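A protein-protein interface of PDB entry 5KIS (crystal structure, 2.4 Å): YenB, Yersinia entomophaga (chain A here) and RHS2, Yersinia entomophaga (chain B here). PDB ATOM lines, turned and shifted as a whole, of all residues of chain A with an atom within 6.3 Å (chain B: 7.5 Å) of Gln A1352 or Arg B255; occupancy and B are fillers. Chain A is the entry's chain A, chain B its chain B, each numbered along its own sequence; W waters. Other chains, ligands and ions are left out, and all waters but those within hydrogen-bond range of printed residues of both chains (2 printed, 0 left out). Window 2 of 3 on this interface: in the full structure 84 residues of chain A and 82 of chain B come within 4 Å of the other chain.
The side-chain amide nitrogen (NE2) of Gln A1354 lies within hydrogen-bond range of the backbone carbonyl oxygen (O) of Tyr B256 (2.7 Å).
The side-chain amide oxygen (OE1) of Gln A1352 sits at hydrogen-bond distance from the guanidinium group (NH1) of Arg B255 (3.0 Å).
The side-chain amide oxygen of Gln A1354 sits at hydrogen-bond distance from the backbone NH of Val B258, 3.1 Å away.
The side-chain carboxylate of Asp A1350 sits at hydrogen-bond distance from the backbone NH of Gln A1352.
OD1 of Asp B257 is in hydrogen-bond range of N of Gly B260 (3.1 Å).
OD2 of Asp A1350 lies within salt-bridge range of NH1 of Arg A1346.
The backbone carbonyl oxygen of Arg A1346 is in hydrogen-bond range of the side-chain amide nitrogen of Gln A1353 (3.0 Å).
O of Leu B242 is in hydrogen-bond range of N of Val B254 (2.7 Å).
The backbone NH (N) of Ser B263 is in hydrogen-bond range of the backbone carbonyl oxygen (O) of Arg B255, 2.8 Å away.
Among the printed residues, pairs that only touch across the chains: Arg A1346 with Leu B242 (3.4 Å), Gln A1354 with Asp B257 (3.5 Å) and Gln A1354 with Arg B255 (3.9 Å).
Of chain B, only Arg B255 comes within 4 Å of Gln A1352.
Printed residues of chain A within 4 Å of Arg B255: Gln A1352 (3.0 Å) and Gln A1354 (3.9 Å).
Printed residues of chain A within 4 Å of Tyr B256: Gln A1354.
Printed residues of chain A within 4 Å of Val B258: Gln A1354.
Of the printed residues of chain B, Gln A1354 touches Arg B255 (3.9 Å), Tyr B256 (2.7 Å), Asp B257 (3.5 Å) and Val B258 (3.1 Å).
Printed residues of chain B within 4 Å of Arg A1346: Leu B242 (3.4 Å).
The nearest residue of chain B that does not touch Gln A1352 is Arg B253 (6.3 Å).
The nearest residue of chain A that does not touch Arg B255 is Arg A1346 (4.7 Å).
The nearest printed residue of chain A that does not touch Leu B242 is Asp A1350 (5.5 Å).
Along chain A the printed residues that touch a printed residue of chain B span positions 1346 to 1354.
Of the 16 printed residues of chain B, 5 touch a printed residue of chain A.
Printed residues of chain B that touch a printed residue of chain A: Leu B242, Arg B255, Tyr B256, Asp B257 and Val B258.
Hydrophobic or aromatic side chains of chain B within 4 Å of the printed part of chain A: Leu B242 and Val B258.
Water W1 bridges NH1 of Arg B255 (2.9 Å) and NH2 of Arg A1346 (3.5 Å).
Water W2 lies within hydrogen-bond range of NH2 of Arg A1346 (2.9 Å) and N of Tyr B256 (3.1 Å).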
ATOM      1  N   PRO A1257     -11.716 -22.633 -21.078  1.00  0.00           N
ATOM      2  CA  PRO A1257     -10.999 -23.585 -20.223  1.00  0.00           C
ATOM      3  C   PRO A1257     -10.636 -24.902 -20.915  1.00  0.00           C
ATOM      4  O   PRO A1257     -11.267 -25.282 -21.901  1.00  0.00           O
ATOM      5  CB  PRO A1257     -11.995 -23.845 -19.091  1.00  0.00           C
ATOM      6  CG  PRO A1257     -12.726 -22.555 -18.959  1.00  0.00           C
ATOM      7  CD  PRO A1257     -12.804 -21.963 -20.340  1.00  0.00           C
ATOM      8  N   ASP A1345      -5.058 -22.710 -13.098  1.00  0.00           N
ATOM      9  CA  ASP A1345      -4.994 -23.204 -11.708  1.00  0.00           C
ATOM     10  C   ASP A1345      -5.118 -24.718 -11.536  1.00  0.00           C
ATOM     11  O   ASP A1345      -4.731 -25.226 -10.496  1.00  0.00           O
ATOM     12  CB  ASP A1345      -5.991 -22.467 -10.784  1.00  0.00           C
ATOM     13  CG  ASP A1345      -7.444 -22.902 -10.959  1.00  0.00           C
ATOM     14  OD1 ASP A1345      -7.824 -23.465 -11.999  1.00  0.00           O
ATOM     15  OD2 ASP A1345      -8.227 -22.618 -10.038  1.00  0.00           O
ATOM     16  N   ARG A1346      -5.652 -25.414 -12.538  1.00  0.00           N
ATOM     17  CA  ARG A1346      -5.715 -26.878 -12.566  1.00  0.00           C
ATOM     18  C   ARG A1346      -5.075 -27.409 -13.831  1.00  0.00           C
ATOM     19  O   ARG A1346      -4.922 -26.680 -14.817  1.00  0.00           O
ATOM     20  CB  ARG A1346      -7.166 -27.355 -12.563  1.00  0.00           C
ATOM     21  CG  ARG A1346      -8.058 -26.781 -11.475  1.00  0.00           C
ATOM     22  CD  ARG A1346      -7.581 -27.157 -10.078  1.00  0.00           C
ATOM     23  NE  ARG A1346      -8.519 -26.687  -9.055  1.00  0.00           N
ATOM     24  CZ  ARG A1346      -9.628 -27.325  -8.677  1.00  0.00           C
ATOM     25  NH1 ARG A1346      -9.967 -28.498  -9.216  1.00  0.00           N
ATOM     26  NH2 ARG A1346     -10.404 -26.780  -7.741  1.00  0.00           N
ATOM     27  N   ASP A1350      -8.587 -31.604 -15.664  1.00  0.00           N
ATOM     28  CA  ASP A1350      -9.562 -31.225 -14.644  1.00  0.00           C
ATOM     29  C   ASP A1350     -10.514 -30.189 -15.219  1.00  0.00           C
ATOM     30  O   ASP A1350     -10.081 -29.115 -15.619  1.00  0.00           O
ATOM     31  CB  ASP A1350      -8.782 -30.642 -13.462  1.00  0.00           C
ATOM     32  CG  ASP A1350      -9.640 -30.261 -12.287  1.00  0.00           C
ATOM     33  OD1 ASP A1350     -10.852 -29.968 -12.430  1.00  0.00           O
ATOM     34  OD2 ASP A1350      -9.052 -30.220 -11.193  1.00  0.00           O
ATOM     35  N   ASP A1351     -11.811 -30.486 -15.224  1.00  0.00           N
ATOM     36  CA  ASP A1351     -12.801 -29.565 -15.819  1.00  0.00           C
ATOM     37  C   ASP A1351     -13.105 -28.310 -14.980  1.00  0.00           C
ATOM     38  O   ASP A1351     -13.800 -27.418 -15.457  1.00  0.00           O
ATOM     39  CB  ASP A1351     -14.105 -30.290 -16.217  1.00  0.00           C
ATOM     40  CG  ASP A1351     -14.871 -30.903 -15.019  1.00  0.00           C
ATOM     41  OD1 ASP A1351     -14.681 -30.524 -13.834  1.00  0.00           O
ATOM     42  OD2 ASP A1351     -15.705 -31.790 -15.288  1.00  0.00           O
ATOM     43  N   GLN A1352     -12.591 -28.254 -13.750  1.00  0.00           N
ATOM     44  CA  GLN A1352     -12.664 -27.047 -12.925  1.00  0.00           C
ATOM     45  C   GLN A1352     -11.631 -25.970 -13.280  1.00  0.00           C
ATOM     46  O   GLN A1352     -11.627 -24.914 -12.653  1.00  0.00           O
ATOM     47  CB  GLN A1352     -12.472 -27.400 -11.437  1.00  0.00           C
ATOM     48  CG  GLN A1352     -13.459 -28.397 -10.872  1.00  0.00           C
ATOM     49  CD  GLN A1352     -14.881 -27.911 -11.018  1.00  0.00           C
ATOM     50  OE1 GLN A1352     -15.283 -26.938 -10.374  1.00  0.00           O
ATOM     51  NE2 GLN A1352     -15.638 -28.557 -11.893  1.00  0.00           N
ATOM     52  N   GLN A1353     -10.746 -26.222 -14.245  1.00  0.00           N
ATOM     53  CA  GLN A1353      -9.698 -25.249 -14.579  1.00  0.00           C
ATOM     54  C   GLN A1353     -10.276 -23.846 -14.867  1.00  0.00           C
ATOM     55  O   GLN A1353     -11.248 -23.703 -15.630  1.00  0.00           O
ATOM     56  CB  GLN A1353      -8.871 -25.737 -15.781  1.00  0.00           C
ATOM     57  CG  GLN A1353      -7.656 -24.880 -16.132  1.00  0.00           C
ATOM     58  CD  GLN A1353      -7.082 -25.225 -17.485  1.00  0.00           C
ATOM     59  OE1 GLN A1353      -7.585 -24.785 -18.519  1.00  0.00           O
ATOM     60  NE2 GLN A1353      -6.016 -26.024 -17.485  1.00  0.00           N
ATOM     61  N   GLN A1354      -9.685 -22.837 -14.227  1.00  0.00           N
ATOM     62  CA  GLN A1354      -9.960 -21.436 -14.525  1.00  0.00           C
ATOM     63  C   GLN A1354      -8.768 -20.806 -15.235  1.00  0.00           C
ATOM     64  O   GLN A1354      -7.632 -21.264 -15.095  1.00  0.00           O
ATOM     65  CB  GLN A1354     -10.245 -20.670 -13.240  1.00  0.00           C
ATOM     66  CG  GLN A1354     -11.406 -21.229 -12.433  1.00  0.00           C
ATOM     67  CD  GLN A1354     -11.658 -20.438 -11.163  1.00  0.00           C
ATOM     68  OE1 GLN A1354     -12.021 -19.266 -11.222  1.00  0.00           O
ATOM     69  NE2 GLN A1354     -11.467 -21.071 -10.010  1.00  0.00           N
ATOM     70  N   VAL B 241      -3.306 -25.657  -1.648  1.00  0.00           N
ATOM     71  CA  VAL B 241      -4.111 -26.734  -1.054  1.00  0.00           C
ATOM     72  C   VAL B 241      -5.573 -26.624  -1.476  1.00  0.00           C
ATOM     73  O   VAL B 241      -6.173 -25.552  -1.379  1.00  0.00           O
ATOM     74  CB  VAL B 241      -4.001 -26.748   0.507  1.00  0.00           C
ATOM     75  CG1 VAL B 241      -5.007 -27.695   1.159  1.00  0.00           C
ATOM     76  CG2 VAL B 241      -2.584 -27.128   0.948  1.00  0.00           C
ATOM     77  N   LEU B 242      -6.122 -27.749  -1.931  1.00  0.00           N
ATOM     78  CA  LEU B 242      -7.537 -27.891  -2.255  1.00  0.00           C
ATOM     79  C   LEU B 242      -8.286 -28.684  -1.169  1.00  0.00           C
ATOM     80  O   LEU B 242      -9.302 -28.195  -0.659  1.00  0.00           O
ATOM     81  CB  LEU B 242      -7.712 -28.595  -3.607  1.00  0.00           C
ATOM     82  CG  LEU B 242      -7.424 -27.799  -4.872  1.00  0.00           C
ATOM     83  CD1 LEU B 242      -7.599 -28.713  -6.063  1.00  0.00           C
ATOM     84  CD2 LEU B 242      -8.344 -26.594  -4.993  1.00  0.00           C
ATOM     85  N   ARG B 253     -12.381 -29.087   2.395  1.00  0.00           N
ATOM     86  CA  ARG B 253     -12.232 -28.759   0.985  1.00  0.00           C
ATOM     87  C   ARG B 253     -12.366 -27.252   0.767  1.00  0.00           C
ATOM     88  O   ARG B 253     -13.187 -26.602   1.399  1.00  0.00           O
ATOM     89  CB  ARG B 253     -13.273 -29.520   0.164  1.00  0.00           C
ATOM     90  CG  ARG B 253     -13.208 -29.273  -1.337  1.00  0.00           C
ATOM     91  CD  ARG B 253     -13.979 -30.323  -2.126  1.00  0.00           C
ATOM     92  NE  ARG B 253     -14.639 -29.715  -3.282  1.00  0.00           N
ATOM     93  CZ  ARG B 253     -15.847 -29.147  -3.290  1.00  0.00           C
ATOM     94  NH1 ARG B 253     -16.618 -29.118  -2.215  1.00  0.00           N
ATOM     95  NH2 ARG B 253     -16.296 -28.605  -4.407  1.00  0.00           N
ATOM     96  N   VAL B 254     -11.547 -26.707  -0.129  1.00  0.00           N
ATOM     97  CA  VAL B 254     -11.639 -25.295  -0.494  1.00  0.00           C
ATOM     98  C   VAL B 254     -11.656 -25.075  -2.004  1.00  0.00           C
ATOM     99  O   VAL B 254     -11.316 -25.965  -2.791  1.00  0.00           O
ATOM    100  CB  VAL B 254     -10.530 -24.453   0.170  1.00  0.00           C
ATOM    101  CG1 VAL B 254     -10.675 -24.513   1.688  1.00  0.00           C
ATOM    102  CG2 VAL B 254      -9.136 -24.903  -0.256  1.00  0.00           C
ATOM    103  N   ARG B 255     -12.109 -23.883  -2.376  1.00  0.00           N
ATOM    104  CA  ARG B 255     -12.211 -23.458  -3.764  1.00  0.00           C
ATOM    105  C   ARG B 255     -11.655 -22.046  -3.894  1.00  0.00           C
ATOM    106  O   ARG B 255     -11.837 -21.209  -2.990  1.00  0.00           O
ATOM    107  CB  ARG B 255     -13.663 -23.485  -4.232  1.00  0.00           C
ATOM    108  CG  ARG B 255     -13.798 -23.198  -5.713  1.00  0.00           C
ATOM    109  CD  ARG B 255     -15.225 -23.268  -6.211  1.00  0.00           C
ATOM    110  NE  ARG B 255     -15.290 -22.733  -7.574  1.00  0.00           N
ATOM    111  CZ  ARG B 255     -14.924 -23.380  -8.689  1.00  0.00           C
ATOM    112  NH1 ARG B 255     -14.466 -24.635  -8.660  1.00  0.00           N
ATOM    113  NH2 ARG B 255     -15.033 -22.760  -9.865  1.00  0.00           N
ATOM    114  N   TYR B 256     -10.976 -21.795  -5.018  1.00  0.00           N
ATOM    115  CA  TYR B 256     -10.358 -20.484  -5.297  1.00  0.00           C
ATOM    116  C   TYR B 256     -11.078 -19.784  -6.451  1.00  0.00           C
ATOM    117  O   TYR B 256     -11.507 -20.432  -7.406  1.00  0.00           O
ATOM    118  CB  TYR B 256      -8.842 -20.629  -5.552  1.00  0.00           C
ATOM    119  CG  TYR B 256      -8.144 -21.182  -4.335  1.00  0.00           C
ATOM    120  CD1 TYR B 256      -7.875 -20.369  -3.234  1.00  0.00           C
ATOM    121  CD2 TYR B 256      -7.811 -22.524  -4.255  1.00  0.00           C
ATOM    122  CE1 TYR B 256      -7.280 -20.873  -2.090  1.00  0.00           C
ATOM    123  CE2 TYR B 256      -7.208 -23.043  -3.122  1.00  0.00           C
ATOM    124  CZ  TYR B 256      -6.948 -22.220  -2.037  1.00  0.00           C
ATOM    125  OH  TYR B 256      -6.350 -22.740  -0.903  1.00  0.00           O
ATOM    126  N   ASP B 257     -11.226 -18.464  -6.332  1.00  0.00           N
ATOM    127  CA  ASP B 257     -11.830 -17.644  -7.394  1.00  0.00           C
ATOM    128  C   ASP B 257     -10.825 -17.430  -8.542  1.00  0.00           C
ATOM    129  O   ASP B 257      -9.686 -17.921  -8.472  1.00  0.00           O
ATOM    130  CB  ASP B 257     -12.403 -16.310  -6.839  1.00  0.00           C
ATOM    131  CG  ASP B 257     -11.347 -15.387  -6.216  1.00  0.00           C
ATOM    132  OD1 ASP B 257     -10.123 -15.564  -6.446  1.00  0.00           O
ATOM    133  OD2 ASP B 257     -11.768 -14.458  -5.488  1.00  0.00           O
ATOM    134  N   VAL B 258     -11.239 -16.698  -9.582  1.00  0.00           N
ATOM    135  CA  VAL B 258     -10.388 -16.458 -10.761  1.00  0.00           C
ATOM    136  C   VAL B 258      -9.116 -15.646 -10.482  1.00  0.00           C
ATOM    137  O   VAL B 258      -8.191 -15.636 -11.308  1.00  0.00           O
ATOM    138  CB  VAL B 258     -11.177 -15.790 -11.906  1.00  0.00           C
ATOM    139  CG1 VAL B 258     -11.497 -14.328 -11.580  1.00  0.00           C
ATOM    140  CG2 VAL B 258     -10.421 -15.927 -13.224  1.00  0.00           C
ATOM    141  N   GLY B 260      -7.342 -16.397  -7.639  1.00  0.00           N
ATOM    142  CA  GLY B 260      -6.606 -17.253  -6.688  1.00  0.00           C
ATOM    143  C   GLY B 260      -6.906 -17.070  -5.195  1.00  0.00           C
ATOM    144  O   GLY B 260      -6.164 -17.586  -4.350  1.00  0.00           O
ATOM    145  N   LEU B 261      -8.000 -16.378  -4.872  1.00  0.00           N
ATOM    146  CA  LEU B 261      -8.431 -16.165  -3.489  1.00  0.00           C
ATOM    147  C   LEU B 261      -9.547 -17.131  -3.083  1.00  0.00           C
ATOM    148  O   LEU B 261     -10.372 -17.524  -3.912  1.00  0.00           O
ATOM    149  CB  LEU B 261      -8.911 -14.722  -3.324  1.00  0.00           C
ATOM    150  CG  LEU B 261      -7.911 -13.683  -3.842  1.00  0.00           C
ATOM    151  CD1 LEU B 261      -8.541 -12.300  -3.865  1.00  0.00           C
ATOM    152  CD2 LEU B 261      -6.620 -13.703  -3.023  1.00  0.00           C
ATOM    153  N   LEU B 262      -9.556 -17.505  -1.801  1.00  0.00           N
ATOM    154  CA  LEU B 262     -10.548 -18.441  -1.227  1.00  0.00           C
ATOM    155  C   LEU B 262     -11.970 -17.914  -1.479  1.00  0.00           C
ATOM    156  O   LEU B 262     -12.302 -16.805  -1.053  1.00  0.00           O
ATOM    157  CB  LEU B 262     -10.281 -18.601   0.289  1.00  0.00           C
ATOM    158  CG  LEU B 262     -10.906 -19.637   1.244  1.00  0.00           C
ATOM    159  CD1 LEU B 262     -12.406 -19.496   1.422  1.00  0.00           C
ATOM    160  CD2 LEU B 262     -10.552 -21.029   0.784  1.00  0.00           C
ATOM    161  N   SER B 263     -12.780 -18.683  -2.208  1.00  0.00           N
ATOM    162  CA  SER B 263     -14.183 -18.309  -2.496  1.00  0.00           C
ATOM    163  C   SER B 263     -15.217 -19.184  -1.776  1.00  0.00           C
ATOM    164  O   SER B 263     -16.352 -18.760  -1.608  1.00  0.00           O
ATOM    165  CB  SER B 263     -14.453 -18.324  -4.008  1.00  0.00           C
ATOM    166  OG  SER B 263     -14.413 -19.641  -4.540  1.00  0.00           O
ATOM    167  N   GLY B 264     -14.842 -20.396  -1.375  1.00  0.00           N
ATOM    168  CA  GLY B 264     -15.728 -21.274  -0.621  1.00  0.00           C
ATOM    169  C   GLY B 264     -14.965 -22.365   0.107  1.00  0.00           C
ATOM    170  O   GLY B 264     -13.846 -22.711  -0.274  1.00  0.00           O
ATOM    171  N   SER B 265     -15.573 -22.891   1.170  1.00  0.00           N
ATOM    172  CA  SER B 265     -15.065 -24.072   1.868  1.00  0.00           C
ATOM    173  C   SER B 265     -16.187 -24.977   2.345  1.00  0.00           C
ATOM    174  O   SER B 265     -17.326 -24.534   2.565  1.00  0.00           O
ATOM    175  CB  SER B 265     -14.146 -23.698   3.049  1.00  0.00           C
ATOM    176  OG  SER B 265     -14.857 -23.177   4.145  1.00  0.00           O
ATOM    177  N   TRP B 266     -15.829 -26.248   2.501  1.00  0.00           N
ATOM    178  CA  TRP B 266     -16.741 -27.321   2.889  1.00  0.00           C
ATOM    179  C   TRP B 266     -16.092 -28.229   3.929  1.00  0.00           C
ATOM    180  O   TRP B 266     -14.870 -28.249   4.084  1.00  0.00           O
ATOM    181  CB  TRP B 266     -17.095 -28.175   1.675  1.00  0.00           C
ATOM    182  CG  TRP B 266     -17.857 -27.470   0.587  1.00  0.00           C
ATOM    183  CD1 TRP B 266     -19.200 -27.524   0.371  1.00  0.00           C
ATOM    184  CD2 TRP B 266     -17.319 -26.630  -0.445  1.00  0.00           C
ATOM    185  NE1 TRP B 266     -19.540 -26.772  -0.723  1.00  0.00           N
ATOM    186  CE2 TRP B 266     -18.406 -26.215  -1.252  1.00  0.00           C
ATOM    187  CE3 TRP B 266     -16.026 -26.195  -0.775  1.00  0.00           C
ATOM    188  CZ2 TRP B 266     -18.243 -25.369  -2.363  1.00  0.00           C
ATOM    189  CZ3 TRP B 266     -15.865 -25.356  -1.882  1.00  0.00           C
ATOM    190  CH2 TRP B 266     -16.973 -24.955  -2.663  1.00  0.00           C
ATOM    191  N   TYR B 283     -14.015  -9.936  -2.156  1.00  0.00           N
ATOM    192  CA  TYR B 283     -12.844  -9.174  -1.702  1.00  0.00           C
ATOM    193  C   TYR B 283     -12.812  -7.751  -2.262  1.00  0.00           C
ATOM    194  O   TYR B 283     -13.348  -7.481  -3.342  1.00  0.00           O
ATOM    195  CB  TYR B 283     -11.562  -9.901  -2.102  1.00  0.00           C
ATOM    196  CG  TYR B 283     -11.420 -11.279  -1.512  1.00  0.00           C
ATOM    197  CD1 TYR B 283     -12.007 -12.385  -2.123  1.00  0.00           C
ATOM    198  CD2 TYR B 283     -10.679 -11.486  -0.352  1.00  0.00           C
ATOM    199  CE1 TYR B 283     -11.873 -13.662  -1.588  1.00  0.00           C
ATOM    200  CE2 TYR B 283     -10.532 -12.755   0.189  1.00  0.00           C
ATOM    201  CZ  TYR B 283     -11.131 -13.839  -0.433  1.00  0.00           C
ATOM    202  OH  TYR B 283     -10.986 -15.093   0.111  1.00  0.00           O
HETATM  203  O   HOH W   1     -13.841 -26.989  -7.160  1.00  0.00           O
HETATM  204  O   HOH W   2     -10.409 -23.879  -7.310  1.00  0.00           O
